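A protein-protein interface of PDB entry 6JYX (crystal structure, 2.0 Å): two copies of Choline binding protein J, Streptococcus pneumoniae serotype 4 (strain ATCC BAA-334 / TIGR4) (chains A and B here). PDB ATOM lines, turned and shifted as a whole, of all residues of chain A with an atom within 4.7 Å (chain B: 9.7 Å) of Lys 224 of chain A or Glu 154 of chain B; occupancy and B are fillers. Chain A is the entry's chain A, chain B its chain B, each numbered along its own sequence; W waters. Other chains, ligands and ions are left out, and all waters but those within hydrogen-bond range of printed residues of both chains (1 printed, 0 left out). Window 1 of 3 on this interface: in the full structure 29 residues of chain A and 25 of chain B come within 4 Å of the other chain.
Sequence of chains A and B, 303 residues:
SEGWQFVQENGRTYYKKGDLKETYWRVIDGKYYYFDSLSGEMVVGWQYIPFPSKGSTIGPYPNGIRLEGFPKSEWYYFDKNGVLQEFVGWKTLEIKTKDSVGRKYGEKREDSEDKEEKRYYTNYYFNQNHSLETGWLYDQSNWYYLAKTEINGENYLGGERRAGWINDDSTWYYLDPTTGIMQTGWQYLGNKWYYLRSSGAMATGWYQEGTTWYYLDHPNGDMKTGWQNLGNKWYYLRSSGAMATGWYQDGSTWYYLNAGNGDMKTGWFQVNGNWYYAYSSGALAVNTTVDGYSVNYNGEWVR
The side-chain carboxylate (OE1) of Glu 154 of chain B is in salt-bridge range of the side-chain amino group (NZ) of Lys 224 of chain A (3.8 Å).
NE2 of Gln 228 of chain A is in hydrogen-bond range of OE2 of Glu 154 of chain B.
The backbone carbonyl oxygen of Tyr 215 of chain A is in hydrogen-bond range of the backbone NH of Lys 224 of chain A, 2.9 Å away.
OD1 of Asp 217 of chain A is in salt-bridge range of NZ of Lys 224 of chain A (3.995 Å).
The side-chain amino group (NZ) of Lys 224 of chain A is in hydrogen-bond range of the side-chain amide oxygen (OE1) of Gln 228 of chain A (2.7 Å).
The backbone carbonyl oxygen (O) of Thr 225 of chain A lies within hydrogen-bond range of the side-chain amide nitrogen (NE2) of Gln 228 of chain A (3.1 Å).
Among the printed residues, merely in contact across the chains: Gln 228 of chain A with Gly 153 of chain B (3.2 Å) and Tyr 215 of chain A with Asn 152 of chain B (3.7 Å).
Printed residues of chain B within 4 Å of Tyr 215 of chain A: Asn 152.
No residue of chain B comes within 4 Å of Met 223 of chain A.
Of the printed residues of chain B, Lys 224 of chain A touches Glu 154 (3.7 Å).
Thr 225 of chain A touches none of the printed residues of chain B.
Printed residues of chain B within 4 Å of Gln 228 of chain A: Gly 153 and Glu 154.
Thr 97 of chain B touches none of the printed residues of chain A.
Of the printed residues of chain A, Asn 152 of chain B touches Tyr 215 (3.7 Å).
Of the printed residues of chain A, Gly 153 of chain B touches Gln 228.
The nearest residue of chain A that does not touch Glu 154 of chain B is Thr 225 of chain A (4.4 Å).
The nearest printed residue of chain A that does not touch Asn 152 of chain B is Lys 224 of chain A (5.3 Å).
Of the 10 printed residues of chain A, 3 touch a printed residue of chain B.
Printed residues of chain A that touch a printed residue of chain B: Tyr 215, Lys 224 and Gln 228.
Hydrophobic or aromatic side chains of chain A within 4 Å of the printed part of chain B: Tyr 215.
Of the 17 printed residues of chain B, 3 touch a printed residue of chain A.
Printed residues of chain B that touch a printed residue of chain A: Asn 152, Gly 153 and Glu 154.
Along chain B the printed residues that touch a printed residue of chain A span positions 152 to 154.
Among the printed residues, 4 pairs touch across the chains.
Among the printed residues, Asp or Glu carboxylates within 4 Å of a Lys or Arg side-chain nitrogen of the other chain: Lys 224 of chain A with Glu 154 of chain B (3.8 Å).
No position is printed for both chains.
Of the 4 pairs that touch across the chains among the printed residues, none has its exchanged pair printed and touching as well.
Water W1 bridges the backbone NH of Thr 225 of chain A and the side-chain carboxylate of Glu 154 of chain B.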
ATOM      1  N   TYR A 215      19.187 -16.621  40.252  1.00  0.00           N
ATOM      2  CA  TYR A 215      19.993 -15.826  39.338  1.00  0.00           C
ATOM      3  C   TYR A 215      19.108 -14.947  38.475  1.00  0.00           C
ATOM      4  O   TYR A 215      18.268 -15.433  37.695  1.00  0.00           O
ATOM      5  CB  TYR A 215      20.948 -16.675  38.476  1.00  0.00           C
ATOM      6  CG  TYR A 215      21.873 -15.804  37.657  1.00  0.00           C
ATOM      7  CD1 TYR A 215      22.997 -15.199  38.238  1.00  0.00           C
ATOM      8  CD2 TYR A 215      21.605 -15.544  36.318  1.00  0.00           C
ATOM      9  CE1 TYR A 215      23.838 -14.388  37.495  1.00  0.00           C
ATOM     10  CE2 TYR A 215      22.442 -14.723  35.564  1.00  0.00           C
ATOM     11  CZ  TYR A 215      23.550 -14.153  36.160  1.00  0.00           C
ATOM     12  OH  TYR A 215      24.371 -13.343  35.421  1.00  0.00           O
ATOM     13  N   ASP A 217      19.036 -12.158  35.522  1.00  0.00           N
ATOM     14  CA  ASP A 217      19.776 -11.743  34.329  1.00  0.00           C
ATOM     15  C   ASP A 217      20.484 -10.420  34.517  1.00  0.00           C
ATOM     16  O   ASP A 217      19.911  -9.466  35.062  1.00  0.00           O
ATOM     17  CB  ASP A 217      18.844 -11.633  33.118  1.00  0.00           C
ATOM     18  CG  ASP A 217      19.608 -11.349  31.816  1.00  0.00           C
ATOM     19  OD1 ASP A 217      19.955 -12.321  31.117  1.00  0.00           O
ATOM     20  OD2 ASP A 217      19.895 -10.160  31.517  1.00  0.00           O
ATOM     21  N   ASP A 222      15.489 -10.370  34.537  1.00  0.00           N
ATOM     22  CA  ASP A 222      14.581 -11.532  34.552  1.00  0.00           C
ATOM     23  C   ASP A 222      15.203 -12.785  35.206  1.00  0.00           C
ATOM     24  O   ASP A 222      16.388 -13.057  35.034  1.00  0.00           O
ATOM     25  CB  ASP A 222      14.068 -11.846  33.146  1.00  0.00           C
ATOM     26  CG  ASP A 222      15.192 -12.044  32.142  1.00  0.00           C
ATOM     27  OD1 ASP A 222      15.915 -11.062  31.864  1.00  0.00           O
ATOM     28  OD2 ASP A 222      15.344 -13.182  31.638  1.00  0.00           O
ATOM     29  N   MET A 223      14.402 -13.520  35.963  1.00  0.00           N
ATOM     30  CA  MET A 223      14.884 -14.685  36.688  1.00  0.00           C
ATOM     31  C   MET A 223      15.118 -15.852  35.729  1.00  0.00           C
ATOM     32  O   MET A 223      14.231 -16.243  34.976  1.00  0.00           O
ATOM     33  CB  MET A 223      13.911 -15.063  37.815  1.00  0.00           C
ATOM     34  CG  MET A 223      14.362 -16.237  38.692  1.00  0.00           C
ATOM     35  SD  MET A 223      13.019 -16.982  39.633  1.00  0.00           S
ATOM     36  CE  MET A 223      12.004 -17.738  38.363  1.00  0.00           C
ATOM     37  N   LYS A 224      16.322 -16.409  35.764  1.00  0.00           N
ATOM     38  CA  LYS A 224      16.676 -17.495  34.863  1.00  0.00           C
ATOM     39  C   LYS A 224      16.247 -18.844  35.423  1.00  0.00           C
ATOM     40  O   LYS A 224      16.280 -19.033  36.635  1.00  0.00           O
ATOM     41  CB  LYS A 224      18.182 -17.488  34.624  1.00  0.00           C
ATOM     42  CG  LYS A 224      18.670 -16.236  33.922  1.00  0.00           C
ATOM     43  CD  LYS A 224      17.970 -16.068  32.575  1.00  0.00           C
ATOM     44  CE  LYS A 224      18.914 -15.506  31.524  1.00  0.00           C
ATOM     45  NZ  LYS A 224      20.204 -16.290  31.500  1.00  0.00           N
ATOM     46  N   THR A 225      15.828 -19.749  34.533  1.00  0.00           N
ATOM     47  CA  THR A 225      15.614 -21.140  34.862  1.00  0.00           C
ATOM     48  C   THR A 225      16.511 -22.023  33.961  1.00  0.00           C
ATOM     49  O   THR A 225      16.997 -21.583  32.907  1.00  0.00           O
ATOM     50  CB  THR A 225      14.133 -21.577  34.647  1.00  0.00           C
ATOM     51  OG1 THR A 225      13.765 -21.340  33.296  1.00  0.00           O
ATOM     52  CG2 THR A 225      13.154 -20.822  35.553  1.00  0.00           C
ATOM     53  N   GLY A 226      16.697 -23.273  34.366  1.00  0.00           N
ATOM     54  CA  GLY A 226      17.422 -24.257  33.556  1.00  0.00           C
ATOM     55  C   GLY A 226      18.924 -24.099  33.695  1.00  0.00           C
ATOM     56  O   GLY A 226      19.411 -23.422  34.605  1.00  0.00           O
ATOM     57  N   GLN A 228      22.500 -22.728  33.225  1.00  0.00           N
ATOM     58  CA  GLN A 228      23.073 -21.430  32.942  1.00  0.00           C
ATOM     59  C   GLN A 228      24.600 -21.509  33.089  1.00  0.00           C
ATOM     60  O   GLN A 228      25.113 -22.054  34.063  1.00  0.00           O
ATOM     61  CB  GLN A 228      22.488 -20.370  33.894  1.00  0.00           C
ATOM     62  CG  GLN A 228      20.948 -20.193  33.764  1.00  0.00           C
ATOM     63  CD  GLN A 228      20.541 -19.624  32.414  1.00  0.00           C
ATOM     64  OE1 GLN A 228      21.196 -18.717  31.907  1.00  0.00           O
ATOM     65  NE2 GLN A 228      19.474 -20.160  31.821  1.00  0.00           N
ATOM     66  N   LEU A 237      19.203 -24.247  37.453  1.00  0.00           N
ATOM     67  CA  LEU A 237      18.137 -23.526  38.155  1.00  0.00           C
ATOM     68  C   LEU A 237      16.786 -24.224  37.909  1.00  0.00           C
ATOM     69  O   LEU A 237      16.368 -24.416  36.775  1.00  0.00           O
ATOM     70  CB  LEU A 237      18.136 -22.047  37.713  1.00  0.00           C
ATOM     71  CG  LEU A 237      19.534 -21.407  37.856  1.00  0.00           C
ATOM     72  CD1 LEU A 237      19.642 -20.115  37.125  1.00  0.00           C
ATOM     73  CD2 LEU A 237      19.871 -21.170  39.296  1.00  0.00           C
ATOM     74  N   GLY A 241      13.109 -21.354  39.734  1.00  0.00           N
ATOM     75  CA  GLY A 241      14.218 -20.396  39.783  1.00  0.00           C
ATOM     76  C   GLY A 241      15.275 -20.782  40.791  1.00  0.00           C
ATOM     77  O   GLY A 241      16.416 -20.294  40.736  1.00  0.00           O
ATOM     78  N   TRP B  75      36.685 -17.577  18.585  1.00  0.00           N
ATOM     79  CA  TRP B  75      35.711 -18.513  18.074  1.00  0.00           C
ATOM     80  C   TRP B  75      36.298 -19.267  16.895  1.00  0.00           C
ATOM     81  O   TRP B  75      36.721 -18.646  15.899  1.00  0.00           O
ATOM     82  CB  TRP B  75      34.443 -17.802  17.579  1.00  0.00           C
ATOM     83  CG  TRP B  75      33.543 -17.232  18.655  1.00  0.00           C
ATOM     84  CD1 TRP B  75      33.463 -15.916  19.047  1.00  0.00           C
ATOM     85  CD2 TRP B  75      32.582 -17.948  19.450  1.00  0.00           C
ATOM     86  NE1 TRP B  75      32.526 -15.786  20.043  1.00  0.00           N
ATOM     87  CE2 TRP B  75      31.957 -17.007  20.296  1.00  0.00           C
ATOM     88  CE3 TRP B  75      32.195 -19.286  19.530  1.00  0.00           C
ATOM     89  CZ2 TRP B  75      30.972 -17.372  21.216  1.00  0.00           C
ATOM     90  CZ3 TRP B  75      31.206 -19.649  20.424  1.00  0.00           C
ATOM     91  CH2 TRP B  75      30.602 -18.693  21.259  1.00  0.00           C
ATOM     92  N   ILE B  95      23.869 -21.609  13.670  1.00  0.00           N
ATOM     93  CA  ILE B  95      23.832 -20.596  14.702  1.00  0.00           C
ATOM     94  C   ILE B  95      24.459 -21.170  15.973  1.00  0.00           C
ATOM     95  O   ILE B  95      24.443 -22.386  16.204  1.00  0.00           O
ATOM     96  CB  ILE B  95      22.372 -20.153  15.031  1.00  0.00           C
ATOM     97  CG1 ILE B  95      21.502 -21.369  15.359  1.00  0.00           C
ATOM     98  CG2 ILE B  95      21.738 -19.386  13.852  1.00  0.00           C
ATOM     99  CD1 ILE B  95      20.142 -20.968  16.081  1.00  0.00           C
ATOM    100  N   LYS B  96      24.984 -20.281  16.790  1.00  0.00           N
ATOM    101  CA  LYS B  96      25.617 -20.662  18.020  1.00  0.00           C
ATOM    102  C   LYS B  96      24.595 -20.665  19.150  1.00  0.00           C
ATOM    103  O   LYS B  96      23.981 -19.617  19.484  1.00  0.00           O
ATOM    104  CB  LYS B  96      26.799 -19.731  18.301  1.00  0.00           C
ATOM    105  CG  LYS B  96      27.953 -19.924  17.318  1.00  0.00           C
ATOM    106  CD  LYS B  96      29.155 -19.013  17.647  1.00  0.00           C
ATOM    107  CE  LYS B  96      28.763 -17.564  17.417  1.00  0.00           C
ATOM    108  NZ  LYS B  96      29.325 -16.670  18.398  1.00  0.00           N
ATOM    109  N   THR B  97      24.388 -21.855  19.707  1.00  0.00           N
ATOM    110  CA  THR B  97      23.543 -22.077  20.885  1.00  0.00           C
ATOM    111  C   THR B  97      24.255 -22.968  21.914  1.00  0.00           C
ATOM    112  O   THR B  97      25.366 -23.487  21.674  1.00  0.00           O
ATOM    113  CB  THR B  97      22.247 -22.836  20.519  1.00  0.00           C
ATOM    114  OG1 THR B  97      22.581 -24.140  20.029  1.00  0.00           O
ATOM    115  CG2 THR B  97      21.427 -22.084  19.455  1.00  0.00           C
ATOM    116  N   LYS B  98      23.579 -23.153  23.044  1.00  0.00           N
ATOM    117  CA  LYS B  98      23.917 -24.180  24.033  1.00  0.00           C
ATOM    118  C   LYS B  98      24.214 -25.527  23.397  1.00  0.00           C
ATOM    119  O   LYS B  98      25.182 -26.190  23.763  1.00  0.00           O
ATOM    120  CB  LYS B  98      22.739 -24.377  24.988  1.00  0.00           C
ATOM    121  CG  LYS B  98      22.504 -23.257  25.958  1.00  0.00           C
ATOM    122  CD  LYS B  98      21.135 -23.374  26.687  1.00  0.00           C
ATOM    123  CE  LYS B  98      21.277 -22.915  28.133  1.00  0.00           C
ATOM    124  NZ  LYS B  98      20.060 -23.141  28.988  1.00  0.00           N
ATOM    125  N   ASP B  99      23.358 -25.945  22.474  1.00  0.00           N
ATOM    126  CA  ASP B  99      23.501 -27.251  21.873  1.00  0.00           C
ATOM    127  C   ASP B  99      24.695 -27.332  20.926  1.00  0.00           C
ATOM    128  O   ASP B  99      25.274 -28.401  20.761  1.00  0.00           O
ATOM    129  CB  ASP B  99      22.227 -27.671  21.124  1.00  0.00           C
ATOM    130  CG  ASP B  99      22.175 -29.186  20.864  1.00  0.00           C
ATOM    131  OD1 ASP B  99      22.584 -29.971  21.759  1.00  0.00           O
ATOM    132  OD2 ASP B  99      21.727 -29.608  19.769  1.00  0.00           O
ATOM    133  N   SER B 100      25.059 -26.212  20.307  1.00  0.00           N
ATOM    134  CA  SER B 100      26.037 -26.239  19.222  1.00  0.00           C
ATOM    135  C   SER B 100      27.446 -25.713  19.566  1.00  0.00           C
ATOM    136  O   SER B 100      28.360 -25.776  18.738  1.00  0.00           O
ATOM    137  CB  SER B 100      25.456 -25.534  17.977  1.00  0.00           C
ATOM    138  OG  SER B 100      25.346 -24.142  18.197  1.00  0.00           O
ATOM    139  N   VAL B 101      27.633 -25.214  20.775  1.00  0.00           N
ATOM    140  CA  VAL B 101      28.920 -24.643  21.166  1.00  0.00           C
ATOM    141  C   VAL B 101      29.536 -25.483  22.302  1.00  0.00           C
ATOM    142  O   VAL B 101      28.814 -25.917  23.200  1.00  0.00           O
ATOM    143  CB  VAL B 101      28.758 -23.189  21.617  1.00  0.00           C
ATOM    144  CG1 VAL B 101      30.080 -22.636  22.242  1.00  0.00           C
ATOM    145  CG2 VAL B 101      28.279 -22.315  20.428  1.00  0.00           C
ATOM    146  N   GLU B 150      29.691 -12.188  23.392  1.00  0.00           N
ATOM    147  CA  GLU B 150      29.020 -12.159  24.680  1.00  0.00           C
ATOM    148  C   GLU B 150      28.532 -13.572  25.008  1.00  0.00           C
ATOM    149  O   GLU B 150      27.453 -13.993  24.538  1.00  0.00           O
ATOM    150  CB  GLU B 150      27.836 -11.160  24.656  1.00  0.00           C
ATOM    151  CG  GLU B 150      27.024 -11.091  25.945  1.00  0.00           C
ATOM    152  CD  GLU B 150      25.644 -10.479  25.747  1.00  0.00           C
ATOM    153  OE1 GLU B 150      25.432  -9.751  24.755  1.00  0.00           O
ATOM    154  OE2 GLU B 150      24.763 -10.722  26.599  1.00  0.00           O
ATOM    155  N   ILE B 151      29.341 -14.298  25.789  1.00  0.00           N
ATOM    156  CA  ILE B 151      28.966 -15.630  26.280  1.00  0.00           C
ATOM    157  C   ILE B 151      28.635 -15.536  27.745  1.00  0.00           C
ATOM    158  O   ILE B 151      29.524 -15.325  28.583  1.00  0.00           O
ATOM    159  CB  ILE B 151      30.093 -16.700  26.203  1.00  0.00           C
ATOM    160  CG1 ILE B 151      31.035 -16.463  25.032  1.00  0.00           C
ATOM    161  CG2 ILE B 151      29.483 -18.120  26.246  1.00  0.00           C
ATOM    162  CD1 ILE B 151      32.240 -15.650  25.454  1.00  0.00           C
ATOM    163  N   ASN B 152      27.361 -15.711  28.054  1.00  0.00           N
ATOM    164  CA  ASN B 152      26.926 -15.737  29.426  1.00  0.00           C
ATOM    165  C   ASN B 152      25.497 -16.221  29.477  1.00  0.00           C
ATOM    166  O   ASN B 152      24.680 -15.878  28.605  1.00  0.00           O
ATOM    167  CB  ASN B 152      27.055 -14.355  30.085  1.00  0.00           C
ATOM    168  CG  ASN B 152      26.903 -14.420  31.593  1.00  0.00           C
ATOM    169  OD1 ASN B 152      27.845 -14.762  32.309  1.00  0.00           O
ATOM    170  ND2 ASN B 152      25.700 -14.128  32.077  1.00  0.00           N
ATOM    171  N   GLY B 153      25.214 -17.038  30.489  1.00  0.00           N
ATOM    172  CA  GLY B 153      23.900 -17.640  30.656  1.00  0.00           C
ATOM    173  C   GLY B 153      23.510 -18.545  29.506  1.00  0.00           C
ATOM    174  O   GLY B 153      23.983 -19.691  29.416  1.00  0.00           O
ATOM    175  N   GLU B 154      22.635 -18.014  28.645  1.00  0.00           N
ATOM    176  CA  GLU B 154      22.169 -18.682  27.431  1.00  0.00           C
ATOM    177  C   GLU B 154      22.718 -18.008  26.154  1.00  0.00           C
ATOM    178  O   GLU B 154      22.457 -18.483  25.030  1.00  0.00           O
ATOM    179  CB  GLU B 154      20.640 -18.674  27.380  1.00  0.00           C
ATOM    180  CG  GLU B 154      19.951 -19.004  28.705  1.00  0.00           C
ATOM    181  CD  GLU B 154      18.513 -18.499  28.772  1.00  0.00           C
ATOM    182  OE1 GLU B 154      18.266 -17.322  28.421  1.00  0.00           O
ATOM    183  OE2 GLU B 154      17.631 -19.279  29.189  1.00  0.00           O
ATOM    184  N   ASN B 155      23.453 -16.902  26.331  1.00  0.00           N
ATOM    185  CA  ASN B 155      24.054 -16.151  25.218  1.00  0.00           C
ATOM    186  C   ASN B 155      25.390 -16.745  24.761  1.00  0.00           C
ATOM    187  O   ASN B 155      26.277 -17.010  25.586  1.00  0.00           O
ATOM    188  CB  ASN B 155      24.271 -14.672  25.592  1.00  0.00           C
ATOM    189  CG  ASN B 155      22.983 -13.835  25.526  1.00  0.00           C
ATOM    190  OD1 ASN B 155      22.035 -14.160  24.806  1.00  0.00           O
ATOM    191  ND2 ASN B 155      22.963 -12.733  26.277  1.00  0.00           N
ATOM    192  N   TYR B 156      25.518 -16.940  23.450  1.00  0.00           N
ATOM    193  CA  TYR B 156      26.743 -17.442  22.820  1.00  0.00           C
ATOM    194  C   TYR B 156      27.018 -16.597  21.597  1.00  0.00           C
ATOM    195  O   TYR B 156      27.328 -17.121  20.507  1.00  0.00           O
ATOM    196  CB  TYR B 156      26.564 -18.894  22.394  1.00  0.00           C
ATOM    197  CG  TYR B 156      26.431 -19.829  23.545  1.00  0.00           C
ATOM    198  CD1 TYR B 156      27.556 -20.434  24.104  1.00  0.00           C
ATOM    199  CD2 TYR B 156      25.185 -20.105  24.095  1.00  0.00           C
ATOM    200  CE1 TYR B 156      27.448 -21.295  25.175  1.00  0.00           C
ATOM    201  CE2 TYR B 156      25.062 -20.962  25.184  1.00  0.00           C
ATOM    202  CZ  TYR B 156      26.202 -21.562  25.707  1.00  0.00           C
ATOM    203  OH  TYR B 156      26.109 -22.414  26.769  1.00  0.00           O
ATOM    204  N   LEU B 157      26.873 -15.290  21.779  1.00  0.00           N
ATOM    205  CA  LEU B 157      26.931 -14.351  20.677  1.00  0.00           C
ATOM    206  C   LEU B 157      28.374 -14.056  20.346  1.00  0.00           C
ATOM    207  O   LEU B 157      29.265 -14.174  21.209  1.00  0.00           O
ATOM    208  CB  LEU B 157      26.187 -13.057  21.037  1.00  0.00           C
ATOM    209  CG  LEU B 157      24.756 -13.211  21.568  1.00  0.00           C
ATOM    210  CD1 LEU B 157      24.354 -11.979  22.369  1.00  0.00           C
ATOM    211  CD2 LEU B 157      23.758 -13.495  20.442  1.00  0.00           C
ATOM    212  N   GLU B 160      28.192 -13.125  14.311  1.00  0.00           N
ATOM    213  CA  GLU B 160      26.997 -13.129  13.484  1.00  0.00           C
ATOM    214  C   GLU B 160      26.929 -11.790  12.762  1.00  0.00           C
ATOM    215  O   GLU B 160      27.102 -10.733  13.393  1.00  0.00           O
ATOM    216  CB  GLU B 160      25.725 -13.278  14.313  1.00  0.00           C
ATOM    217  CG  GLU B 160      25.503 -14.653  14.989  1.00  0.00           C
ATOM    218  CD  GLU B 160      26.232 -14.780  16.331  1.00  0.00           C
ATOM    219  OE1 GLU B 160      26.817 -13.774  16.823  1.00  0.00           O
ATOM    220  OE2 GLU B 160      26.226 -15.906  16.891  1.00  0.00           O
HETATM  221  O   HOH W   1      15.932 -18.650  31.685  1.00  0.00           O
